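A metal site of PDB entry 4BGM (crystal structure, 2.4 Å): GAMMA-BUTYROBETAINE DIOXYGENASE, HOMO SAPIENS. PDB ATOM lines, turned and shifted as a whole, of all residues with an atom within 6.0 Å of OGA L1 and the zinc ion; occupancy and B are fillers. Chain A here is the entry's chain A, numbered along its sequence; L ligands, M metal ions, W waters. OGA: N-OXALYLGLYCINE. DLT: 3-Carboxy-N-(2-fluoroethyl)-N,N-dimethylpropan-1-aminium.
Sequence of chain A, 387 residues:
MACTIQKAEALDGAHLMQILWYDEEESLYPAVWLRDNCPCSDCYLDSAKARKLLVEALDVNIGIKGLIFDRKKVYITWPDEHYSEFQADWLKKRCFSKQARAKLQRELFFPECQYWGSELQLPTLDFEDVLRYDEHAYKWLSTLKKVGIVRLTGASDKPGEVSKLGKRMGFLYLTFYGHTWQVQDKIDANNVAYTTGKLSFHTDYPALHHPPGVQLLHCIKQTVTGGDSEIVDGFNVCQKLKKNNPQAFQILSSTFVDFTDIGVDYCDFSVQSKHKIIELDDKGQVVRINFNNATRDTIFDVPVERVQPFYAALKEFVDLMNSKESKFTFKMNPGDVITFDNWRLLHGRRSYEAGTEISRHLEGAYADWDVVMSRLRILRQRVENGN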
ATOM      1  N   TRP A 181      -1.974  -9.962 -20.417  1.00  0.00           N
ATOM      2  CA  TRP A 181      -2.725 -10.632 -21.448  1.00  0.00           C
ATOM      3  C   TRP A 181      -2.019 -10.471 -22.767  1.00  0.00           C
ATOM      4  O   TRP A 181      -1.247  -9.527 -22.949  1.00  0.00           O
ATOM      5  CB  TRP A 181      -4.160 -10.101 -21.561  1.00  0.00           C
ATOM      6  CG  TRP A 181      -4.353  -8.725 -21.094  1.00  0.00           C
ATOM      7  CD1 TRP A 181      -4.718  -8.336 -19.848  1.00  0.00           C
ATOM      8  CD2 TRP A 181      -4.213  -7.526 -21.870  1.00  0.00           C
ATOM      9  NE1 TRP A 181      -4.806  -6.966 -19.790  1.00  0.00           N
ATOM     10  CE2 TRP A 181      -4.498  -6.444 -21.021  1.00  0.00           C
ATOM     11  CE3 TRP A 181      -3.872  -7.254 -23.206  1.00  0.00           C
ATOM     12  CZ2 TRP A 181      -4.467  -5.136 -21.461  1.00  0.00           C
ATOM     13  CZ3 TRP A 181      -3.833  -5.950 -23.634  1.00  0.00           C
ATOM     14  CH2 TRP A 181      -4.138  -4.914 -22.768  1.00  0.00           C
ATOM     15  N   VAL A 183      -2.076 -10.023 -26.796  1.00  0.00           N
ATOM     16  CA  VAL A 183      -2.853  -9.519 -27.941  1.00  0.00           C
ATOM     17  C   VAL A 183      -2.266 -10.104 -29.212  1.00  0.00           C
ATOM     18  O   VAL A 183      -1.206  -9.697 -29.669  1.00  0.00           O
ATOM     19  CB  VAL A 183      -2.848  -7.985 -28.031  1.00  0.00           C
ATOM     20  CG1 VAL A 183      -3.674  -7.483 -29.214  1.00  0.00           C
ATOM     21  CG2 VAL A 183      -3.386  -7.407 -26.742  1.00  0.00           C
ATOM     22  N   ASN A 191     -12.627 -12.172 -27.887  1.00  0.00           N
ATOM     23  CA  ASN A 191     -12.552 -10.710 -27.905  1.00  0.00           C
ATOM     24  C   ASN A 191     -12.006 -10.203 -29.242  1.00  0.00           C
ATOM     25  O   ASN A 191     -11.055 -10.764 -29.759  1.00  0.00           O
ATOM     26  CB  ASN A 191     -11.669 -10.242 -26.741  1.00  0.00           C
ATOM     27  CG  ASN A 191     -11.832  -8.753 -26.412  1.00  0.00           C
ATOM     28  OD1 ASN A 191     -11.364  -7.907 -27.145  1.00  0.00           O
ATOM     29  ND2 ASN A 191     -12.456  -8.455 -25.296  1.00  0.00           N
ATOM     30  N   ALA A 193     -10.173  -7.855 -30.028  1.00  0.00           N
ATOM     31  CA  ALA A 193      -8.749  -7.519 -29.954  1.00  0.00           C
ATOM     32  C   ALA A 193      -7.868  -8.698 -30.366  1.00  0.00           C
ATOM     33  O   ALA A 193      -6.763  -8.517 -30.876  1.00  0.00           O
ATOM     34  CB  ALA A 193      -8.411  -7.059 -28.559  1.00  0.00           C
ATOM     35  N   TYR A 194      -8.370  -9.912 -30.132  1.00  0.00           N
ATOM     36  CA  TYR A 194      -7.673 -11.136 -30.441  1.00  0.00           C
ATOM     37  C   TYR A 194      -8.014 -11.710 -31.875  1.00  0.00           C
ATOM     38  O   TYR A 194      -8.263 -12.910 -32.057  1.00  0.00           O
ATOM     39  CB  TYR A 194      -7.975 -12.166 -29.337  1.00  0.00           C
ATOM     40  CG  TYR A 194      -7.653 -11.702 -27.894  1.00  0.00           C
ATOM     41  CD1 TYR A 194      -6.665 -10.708 -27.618  1.00  0.00           C
ATOM     42  CD2 TYR A 194      -8.292 -12.302 -26.794  1.00  0.00           C
ATOM     43  CE1 TYR A 194      -6.373 -10.323 -26.311  1.00  0.00           C
ATOM     44  CE2 TYR A 194      -7.980 -11.923 -25.495  1.00  0.00           C
ATOM     45  CZ  TYR A 194      -7.024 -10.948 -25.263  1.00  0.00           C
ATOM     46  OH  TYR A 194      -6.742 -10.601 -23.978  1.00  0.00           O
ATOM     47  N   LEU A 199      -9.356  -2.201 -35.163  1.00  0.00           N
ATOM     48  CA  LEU A 199     -10.031  -1.696 -33.995  1.00  0.00           C
ATOM     49  C   LEU A 199     -10.097  -0.195 -34.188  1.00  0.00           C
ATOM     50  O   LEU A 199      -9.067   0.442 -34.328  1.00  0.00           O
ATOM     51  CB  LEU A 199      -9.243  -2.029 -32.729  1.00  0.00           C
ATOM     52  CG  LEU A 199      -8.975  -3.507 -32.535  1.00  0.00           C
ATOM     53  CD1 LEU A 199      -8.006  -3.696 -31.394  1.00  0.00           C
ATOM     54  CD2 LEU A 199     -10.267  -4.269 -32.253  1.00  0.00           C
ATOM     55  N   HIS A 202     -11.335   3.373 -29.273  1.00  0.00           N
ATOM     56  CA  HIS A 202     -12.070   2.921 -28.108  1.00  0.00           C
ATOM     57  C   HIS A 202     -11.254   3.185 -26.852  1.00  0.00           C
ATOM     58  O   HIS A 202     -10.040   3.466 -26.940  1.00  0.00           O
ATOM     59  CB  HIS A 202     -12.363   1.403 -28.204  1.00  0.00           C
ATOM     60  CG  HIS A 202     -11.134   0.539 -28.242  1.00  0.00           C
ATOM     61  ND1 HIS A 202     -10.338   0.445 -29.353  1.00  0.00           N
ATOM     62  CD2 HIS A 202     -10.572  -0.261 -27.310  1.00  0.00           C
ATOM     63  CE1 HIS A 202      -9.334  -0.384 -29.112  1.00  0.00           C
ATOM     64  NE2 HIS A 202      -9.450  -0.817 -27.872  1.00  0.00           N
ATOM     65  N   THR A 203     -11.904   3.075 -25.706  1.00  0.00           N
ATOM     66  CA  THR A 203     -11.209   2.925 -24.445  1.00  0.00           C
ATOM     67  C   THR A 203     -11.379   1.491 -24.097  1.00  0.00           C
ATOM     68  O   THR A 203     -12.282   0.871 -24.596  1.00  0.00           O
ATOM     69  CB  THR A 203     -11.783   3.832 -23.326  1.00  0.00           C
ATOM     70  OG1 THR A 203     -13.157   3.524 -23.039  1.00  0.00           O
ATOM     71  CG2 THR A 203     -11.674   5.280 -23.734  1.00  0.00           C
ATOM     72  N   ASP A 204     -10.513   0.958 -23.242  1.00  0.00           N
ATOM     73  CA  ASP A 204     -10.564  -0.447 -22.835  1.00  0.00           C
ATOM     74  C   ASP A 204     -11.408  -0.608 -21.598  1.00  0.00           C
ATOM     75  O   ASP A 204     -11.358   0.213 -20.685  1.00  0.00           O
ATOM     76  CB  ASP A 204      -9.169  -0.982 -22.546  1.00  0.00           C
ATOM     77  CG  ASP A 204      -8.538  -1.683 -23.750  1.00  0.00           C
ATOM     78  OD1 ASP A 204      -8.843  -1.314 -24.932  1.00  0.00           O
ATOM     79  OD2 ASP A 204      -7.689  -2.565 -23.471  1.00  0.00           O
ATOM     80  N   GLN A 215      -3.083   1.999 -19.173  1.00  0.00           N
ATOM     81  CA  GLN A 215      -2.878   0.805 -19.973  1.00  0.00           C
ATOM     82  C   GLN A 215      -1.440   0.735 -20.389  1.00  0.00           C
ATOM     83  O   GLN A 215      -0.824   1.743 -20.726  1.00  0.00           O
ATOM     84  CB  GLN A 215      -3.799   0.791 -21.207  1.00  0.00           C
ATOM     85  CG  GLN A 215      -3.659  -0.461 -22.077  1.00  0.00           C
ATOM     86  CD  GLN A 215      -4.721  -0.570 -23.181  1.00  0.00           C
ATOM     87  OE1 GLN A 215      -4.517  -1.242 -24.207  1.00  0.00           O
ATOM     88  NE2 GLN A 215      -5.833   0.096 -22.982  1.00  0.00           N
ATOM     89  N   LEU A 217       0.998  -1.488 -23.085  1.00  0.00           N
ATOM     90  CA  LEU A 217       1.034  -2.381 -24.236  1.00  0.00           C
ATOM     91  C   LEU A 217       2.478  -2.452 -24.692  1.00  0.00           C
ATOM     92  O   LEU A 217       3.113  -1.423 -24.966  1.00  0.00           O
ATOM     93  CB  LEU A 217       0.209  -1.838 -25.399  1.00  0.00           C
ATOM     94  CG  LEU A 217      -1.288  -2.125 -25.516  1.00  0.00           C
ATOM     95  CD1 LEU A 217      -1.744  -1.671 -26.904  1.00  0.00           C
ATOM     96  CD2 LEU A 217      -1.627  -3.586 -25.325  1.00  0.00           C
ATOM     97  N   GLY A 227      -1.170  -3.198 -38.775  1.00  0.00           N
ATOM     98  CA  GLY A 227      -1.024  -3.150 -37.326  1.00  0.00           C
ATOM     99  C   GLY A 227      -0.577  -1.829 -36.740  1.00  0.00           C
ATOM    100  O   GLY A 227      -0.101  -1.778 -35.605  1.00  0.00           O
ATOM    101  N   ASP A 228      -0.716  -0.742 -37.508  1.00  0.00           N
ATOM    102  CA  ASP A 228      -0.303   0.555 -37.039  1.00  0.00           C
ATOM    103  C   ASP A 228      -1.169   0.957 -35.859  1.00  0.00           C
ATOM    104  O   ASP A 228      -2.328   0.605 -35.812  1.00  0.00           O
ATOM    105  CB  ASP A 228      -0.435   1.602 -38.149  1.00  0.00           C
ATOM    106  CG  ASP A 228       0.561   1.405 -39.269  1.00  0.00           C
ATOM    107  OD1 ASP A 228       0.441   0.397 -39.969  1.00  0.00           O
ATOM    108  OD2 ASP A 228       1.450   2.254 -39.452  1.00  0.00           O
ATOM    109  N   SER A 229      -0.598   1.685 -34.916  1.00  0.00           N
ATOM    110  CA  SER A 229      -1.349   2.177 -33.781  1.00  0.00           C
ATOM    111  C   SER A 229      -1.912   3.522 -34.119  1.00  0.00           C
ATOM    112  O   SER A 229      -1.335   4.248 -34.936  1.00  0.00           O
ATOM    113  CB  SER A 229      -0.474   2.271 -32.544  1.00  0.00           C
ATOM    114  OG  SER A 229       0.088   1.024 -32.247  1.00  0.00           O
ATOM    115  N   ASN A 292     -16.180   1.558 -25.938  1.00  0.00           N
ATOM    116  CA  ASN A 292     -15.648   0.560 -26.861  1.00  0.00           C
ATOM    117  C   ASN A 292     -16.844   0.052 -27.699  1.00  0.00           C
ATOM    118  O   ASN A 292     -17.814  -0.424 -27.157  1.00  0.00           O
ATOM    119  CB  ASN A 292     -14.927  -0.554 -26.095  1.00  0.00           C
ATOM    120  CG  ASN A 292     -14.416  -1.661 -27.000  1.00  0.00           C
ATOM    121  OD1 ASN A 292     -14.795  -1.756 -28.171  1.00  0.00           O
ATOM    122  ND2 ASN A 292     -13.571  -2.533 -26.460  1.00  0.00           N
ATOM    123  N   MET A 332       4.294   0.539 -33.641  1.00  0.00           N
ATOM    124  CA  MET A 332       5.138   0.036 -32.577  1.00  0.00           C
ATOM    125  C   MET A 332       6.131  -0.972 -33.166  1.00  0.00           C
ATOM    126  O   MET A 332       5.795  -1.722 -34.082  1.00  0.00           O
ATOM    127  CB  MET A 332       4.292  -0.638 -31.498  1.00  0.00           C
ATOM    128  CG  MET A 332       3.299   0.279 -30.777  1.00  0.00           C
ATOM    129  SD  MET A 332       2.499  -0.575 -29.376  1.00  0.00           S
ATOM    130  CE  MET A 332       3.920  -0.637 -28.287  1.00  0.00           C
ATOM    131  N   ASN A 342      -6.016   5.607 -20.114  1.00  0.00           N
ATOM    132  CA  ASN A 342      -7.157   4.917 -20.700  1.00  0.00           C
ATOM    133  C   ASN A 342      -8.504   5.552 -20.304  1.00  0.00           C
ATOM    134  O   ASN A 342      -9.570   5.126 -20.748  1.00  0.00           O
ATOM    135  CB  ASN A 342      -7.093   3.439 -20.305  1.00  0.00           C
ATOM    136  CG  ASN A 342      -8.203   2.613 -20.925  1.00  0.00           C
ATOM    137  OD1 ASN A 342      -8.193   2.337 -22.116  1.00  0.00           O
ATOM    138  ND2 ASN A 342      -9.143   2.187 -20.106  1.00  0.00           N
ATOM    139  N   HIS A 347      -7.810   4.646 -28.316  1.00  0.00           N
ATOM    140  CA  HIS A 347      -6.755   4.082 -29.091  1.00  0.00           C
ATOM    141  C   HIS A 347      -7.272   3.049 -30.063  1.00  0.00           C
ATOM    142  O   HIS A 347      -8.392   2.550 -29.918  1.00  0.00           O
ATOM    143  CB  HIS A 347      -5.724   3.466 -28.179  1.00  0.00           C
ATOM    144  CG  HIS A 347      -6.253   2.340 -27.362  1.00  0.00           C
ATOM    145  ND1 HIS A 347      -7.016   2.528 -26.236  1.00  0.00           N
ATOM    146  CD2 HIS A 347      -6.137   0.998 -27.527  1.00  0.00           C
ATOM    147  CE1 HIS A 347      -7.351   1.358 -25.733  1.00  0.00           C
ATOM    148  NE2 HIS A 347      -6.836   0.412 -26.497  1.00  0.00           N
ATOM    149  N   GLY A 348      -6.441   2.701 -31.026  1.00  0.00           N
ATOM    150  CA  GLY A 348      -6.887   1.903 -32.111  1.00  0.00           C
ATOM    151  C   GLY A 348      -5.770   1.251 -32.865  1.00  0.00           C
ATOM    152  O   GLY A 348      -4.605   1.481 -32.617  1.00  0.00           O
ATOM    153  N   ARG A 349      -6.155   0.414 -33.809  1.00  0.00           N
ATOM    154  CA  ARG A 349      -5.207  -0.413 -34.518  1.00  0.00           C
ATOM    155  C   ARG A 349      -5.753  -0.713 -35.925  1.00  0.00           C
ATOM    156  O   ARG A 349      -6.962  -0.973 -36.099  1.00  0.00           O
ATOM    157  CB  ARG A 349      -4.985  -1.710 -33.746  1.00  0.00           C
ATOM    158  CG  ARG A 349      -4.414  -2.832 -34.581  1.00  0.00           C
ATOM    159  CD  ARG A 349      -4.547  -4.177 -33.924  1.00  0.00           C
ATOM    160  NE  ARG A 349      -5.769  -4.927 -34.198  1.00  0.00           N
ATOM    161  CZ  ARG A 349      -6.192  -5.929 -33.426  1.00  0.00           C
ATOM    162  NH1 ARG A 349      -5.526  -6.254 -32.320  1.00  0.00           N
ATOM    163  NH2 ARG A 349      -7.297  -6.604 -33.723  1.00  0.00           N
ATOM    164  N   ARG A 360       2.127 -11.287 -35.166  1.00  0.00           N
ATOM    165  CA  ARG A 360       1.948 -10.103 -34.342  1.00  0.00           C
ATOM    166  C   ARG A 360       1.536 -10.471 -32.915  1.00  0.00           C
ATOM    167  O   ARG A 360       0.583 -11.224 -32.712  1.00  0.00           O
ATOM    168  CB  ARG A 360       0.914  -9.170 -34.973  1.00  0.00           C
ATOM    169  CG  ARG A 360       1.063  -7.724 -34.535  1.00  0.00           C
ATOM    170  CD  ARG A 360      -0.198  -6.980 -34.845  1.00  0.00           C
ATOM    171  NE  ARG A 360      -0.157  -5.566 -34.484  1.00  0.00           N
ATOM    172  CZ  ARG A 360      -0.891  -4.987 -33.529  1.00  0.00           C
ATOM    173  NH1 ARG A 360      -1.709  -5.688 -32.759  1.00  0.00           N
ATOM    174  NH2 ARG A 360      -0.799  -3.679 -33.322  1.00  0.00           N
ATOM    175  N   LEU A 362       1.395  -8.529 -28.903  1.00  0.00           N
ATOM    176  CA  LEU A 362       1.616  -7.542 -27.865  1.00  0.00           C
ATOM    177  C   LEU A 362       1.317  -8.191 -26.510  1.00  0.00           C
ATOM    178  O   LEU A 362       0.513  -9.141 -26.414  1.00  0.00           O
ATOM    179  CB  LEU A 362       0.725  -6.320 -28.050  1.00  0.00           C
ATOM    180  CG  LEU A 362       0.560  -5.611 -29.396  1.00  0.00           C
ATOM    181  CD1 LEU A 362      -0.379  -4.441 -29.255  1.00  0.00           C
ATOM    182  CD2 LEU A 362       1.879  -5.109 -29.976  1.00  0.00           C
ATOM    183  N   TYR A 366      -2.934  -3.481 -17.129  1.00  0.00           N
ATOM    184  CA  TYR A 366      -3.586  -2.270 -16.661  1.00  0.00           C
ATOM    185  C   TYR A 366      -3.097  -1.927 -15.263  1.00  0.00           C
ATOM    186  O   TYR A 366      -2.539  -2.778 -14.564  1.00  0.00           O
ATOM    187  CB  TYR A 366      -5.086  -2.502 -16.556  1.00  0.00           C
ATOM    188  CG  TYR A 366      -5.785  -2.838 -17.835  1.00  0.00           C
ATOM    189  CD1 TYR A 366      -5.728  -1.986 -18.955  1.00  0.00           C
ATOM    190  CD2 TYR A 366      -6.538  -3.999 -17.942  1.00  0.00           C
ATOM    191  CE1 TYR A 366      -6.405  -2.304 -20.119  1.00  0.00           C
ATOM    192  CE2 TYR A 366      -7.218  -4.317 -19.087  1.00  0.00           C
ATOM    193  CZ  TYR A 366      -7.161  -3.477 -20.166  1.00  0.00           C
ATOM    194  OH  TYR A 366      -7.841  -3.848 -21.300  1.00  0.00           O
HETATM  195  C1  OGA L   1      -6.706  -3.839 -27.510  1.00  0.00           C
HETATM  196  C2  OGA L   1      -6.012  -2.898 -28.371  1.00  0.00           C
HETATM  197  C4  OGA L   1      -4.313  -2.441 -29.975  1.00  0.00           C
HETATM  198  C5  OGA L   1      -3.366  -3.174 -30.866  1.00  0.00           C
HETATM  199  O1  OGA L   1      -7.615  -3.421 -26.773  1.00  0.00           O
HETATM  200  O2  OGA L   1      -6.330  -5.048 -27.515  1.00  0.00           O
HETATM  201  O2' OGA L   1      -6.285  -1.705 -28.371  1.00  0.00           O
HETATM  202  O3  OGA L   1      -2.532  -2.458 -31.421  1.00  0.00           O
HETATM  203  N1  OGA L   1      -5.032  -3.363 -29.118  1.00  0.00           N
HETATM  204  O4  OGA L   1      -3.451  -4.422 -31.043  1.00  0.00           O
HETATM  205  CAF DLT L   2      -8.161  -7.732 -22.850  1.00  0.00           C
HETATM  206  CAE DLT L   2      -7.734  -7.021 -21.575  1.00  0.00           C
HETATM  207  CAA DLT L   2      -7.312  -6.089 -24.431  1.00  0.00           C
HETATM  208  CAH DLT L   2      -8.934  -7.731 -25.063  1.00  0.00           C
HETATM  209  CAJ DLT L   2      -9.619  -5.962 -23.562  1.00  0.00           C
HETATM  210  CAK DLT L   2     -10.253  -5.199 -24.737  1.00  0.00           C
HETATM  211  CAL DLT L   2     -11.102  -4.024 -24.269  1.00  0.00           C
HETATM  212  CAM DLT L   2     -12.525  -4.388 -24.000  1.00  0.00           C
HETATM  213  N3  DLT L   2      -8.496  -6.834 -23.970  1.00  0.00           N
HETATM  214  OAC DLT L   2     -12.959  -5.560 -24.038  1.00  0.00           O
HETATM  215  F26 DLT L   2      -8.835  -6.661 -20.847  1.00  0.00           F
HETATM  216  OAB DLT L   2     -13.254  -3.428 -23.703  1.00  0.00           O
HETATM  217 ZN    ZN M   1      -7.706  -1.523 -26.638  1.00  0.00          ZN
HETATM  218  O   HOH W   1      -2.378   0.174 -31.132  1.00  0.00           O
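NH1 of Arg 360 lies within salt-bridge range of O4 of OGA L1, 2.8 Å away. The guanidinium group (NH1) of Arg 349 lies within salt-bridge range of an oxygen (O4) of OGA L1, at 3.0 Å. The side-chain amide nitrogen of Asn 191 is in hydrogen-bond range of an oxygen (OAC) of DLT L2, at 3.2 Å. ND2 of Asn 292 sits at hydrogen-bond distance from OAB of DLT L2 (2.9 Å).
The side-chain carboxylate (OD2) of Asp 204 sits at hydrogen-bond distance from the side-chain amide nitrogen (NE2) of Gln 215, at 3.3 Å. The side-chain carboxylate (OD2) of Asp 204 sits at hydrogen-bond distance from the side-chain hydroxyl (OH) of Tyr 366 (2.5 Å). N of Asp 204 lies within hydrogen-bond range of OD1 of Asn 342 (2.9 Å). The guanidinium group (NH2) of Arg 360 sits at hydrogen-bond distance from the backbone carbonyl oxygen (O) of Gly 227, 3.1 Å away. The guanidinium group of Arg 349 is in hydrogen-bond range of the backbone carbonyl oxygen of Ala 193 (3.0 Å). N of Leu 199 is in hydrogen-bond range of O of Arg 349 (2.8 Å). The backbone NH (N) of Ala 193 lies close to the side-chain amide oxygen (OD1) of Asn 191 (3.1 Å). The backbone NH (N) of Val 183 sits at hydrogen-bond distance from the backbone carbonyl oxygen (O) of Leu 362 (2.8 Å).
Residues that only touch OGA L1: Ala 193 (3.1 Å), Leu 362 (3.6 Å), Val 183 (3.6 Å) and Leu 199 (3.7 Å). Hydrophobic or aromatic side chains that line OGA L1: Val 183, Ala 193, Leu 199, His 202, His 347 and Leu 362. Along chain A the residues within 4 Å of OGA L1 span positions 183 to 362.
Within 4 Å of the zinc ion: His 202, Asp 204 and His 347. The nearest printed residue that does not touch the zinc ion is Gln 215 (4.02 Å).
The zinc ion is bound by an oxygen (O1) of OGA L1 (1.9 Å), the side-chain carboxylate of Asp 204 (2.1 Å), a ring nitrogen (NE2) of His 347 (2.1 Å), an oxygen (O2') of OGA L1 (2.2 Å) and a ring nitrogen (NE2) of His 202 (2.3 Å). The zinc ion has five donor atoms within binding distance.
Water W1 lies within hydrogen-bond range of O3 of OGA L1 (2.7 Å), OG of Ser 229 (2.8 Å) and O of Gly 348 (3.0 Å).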
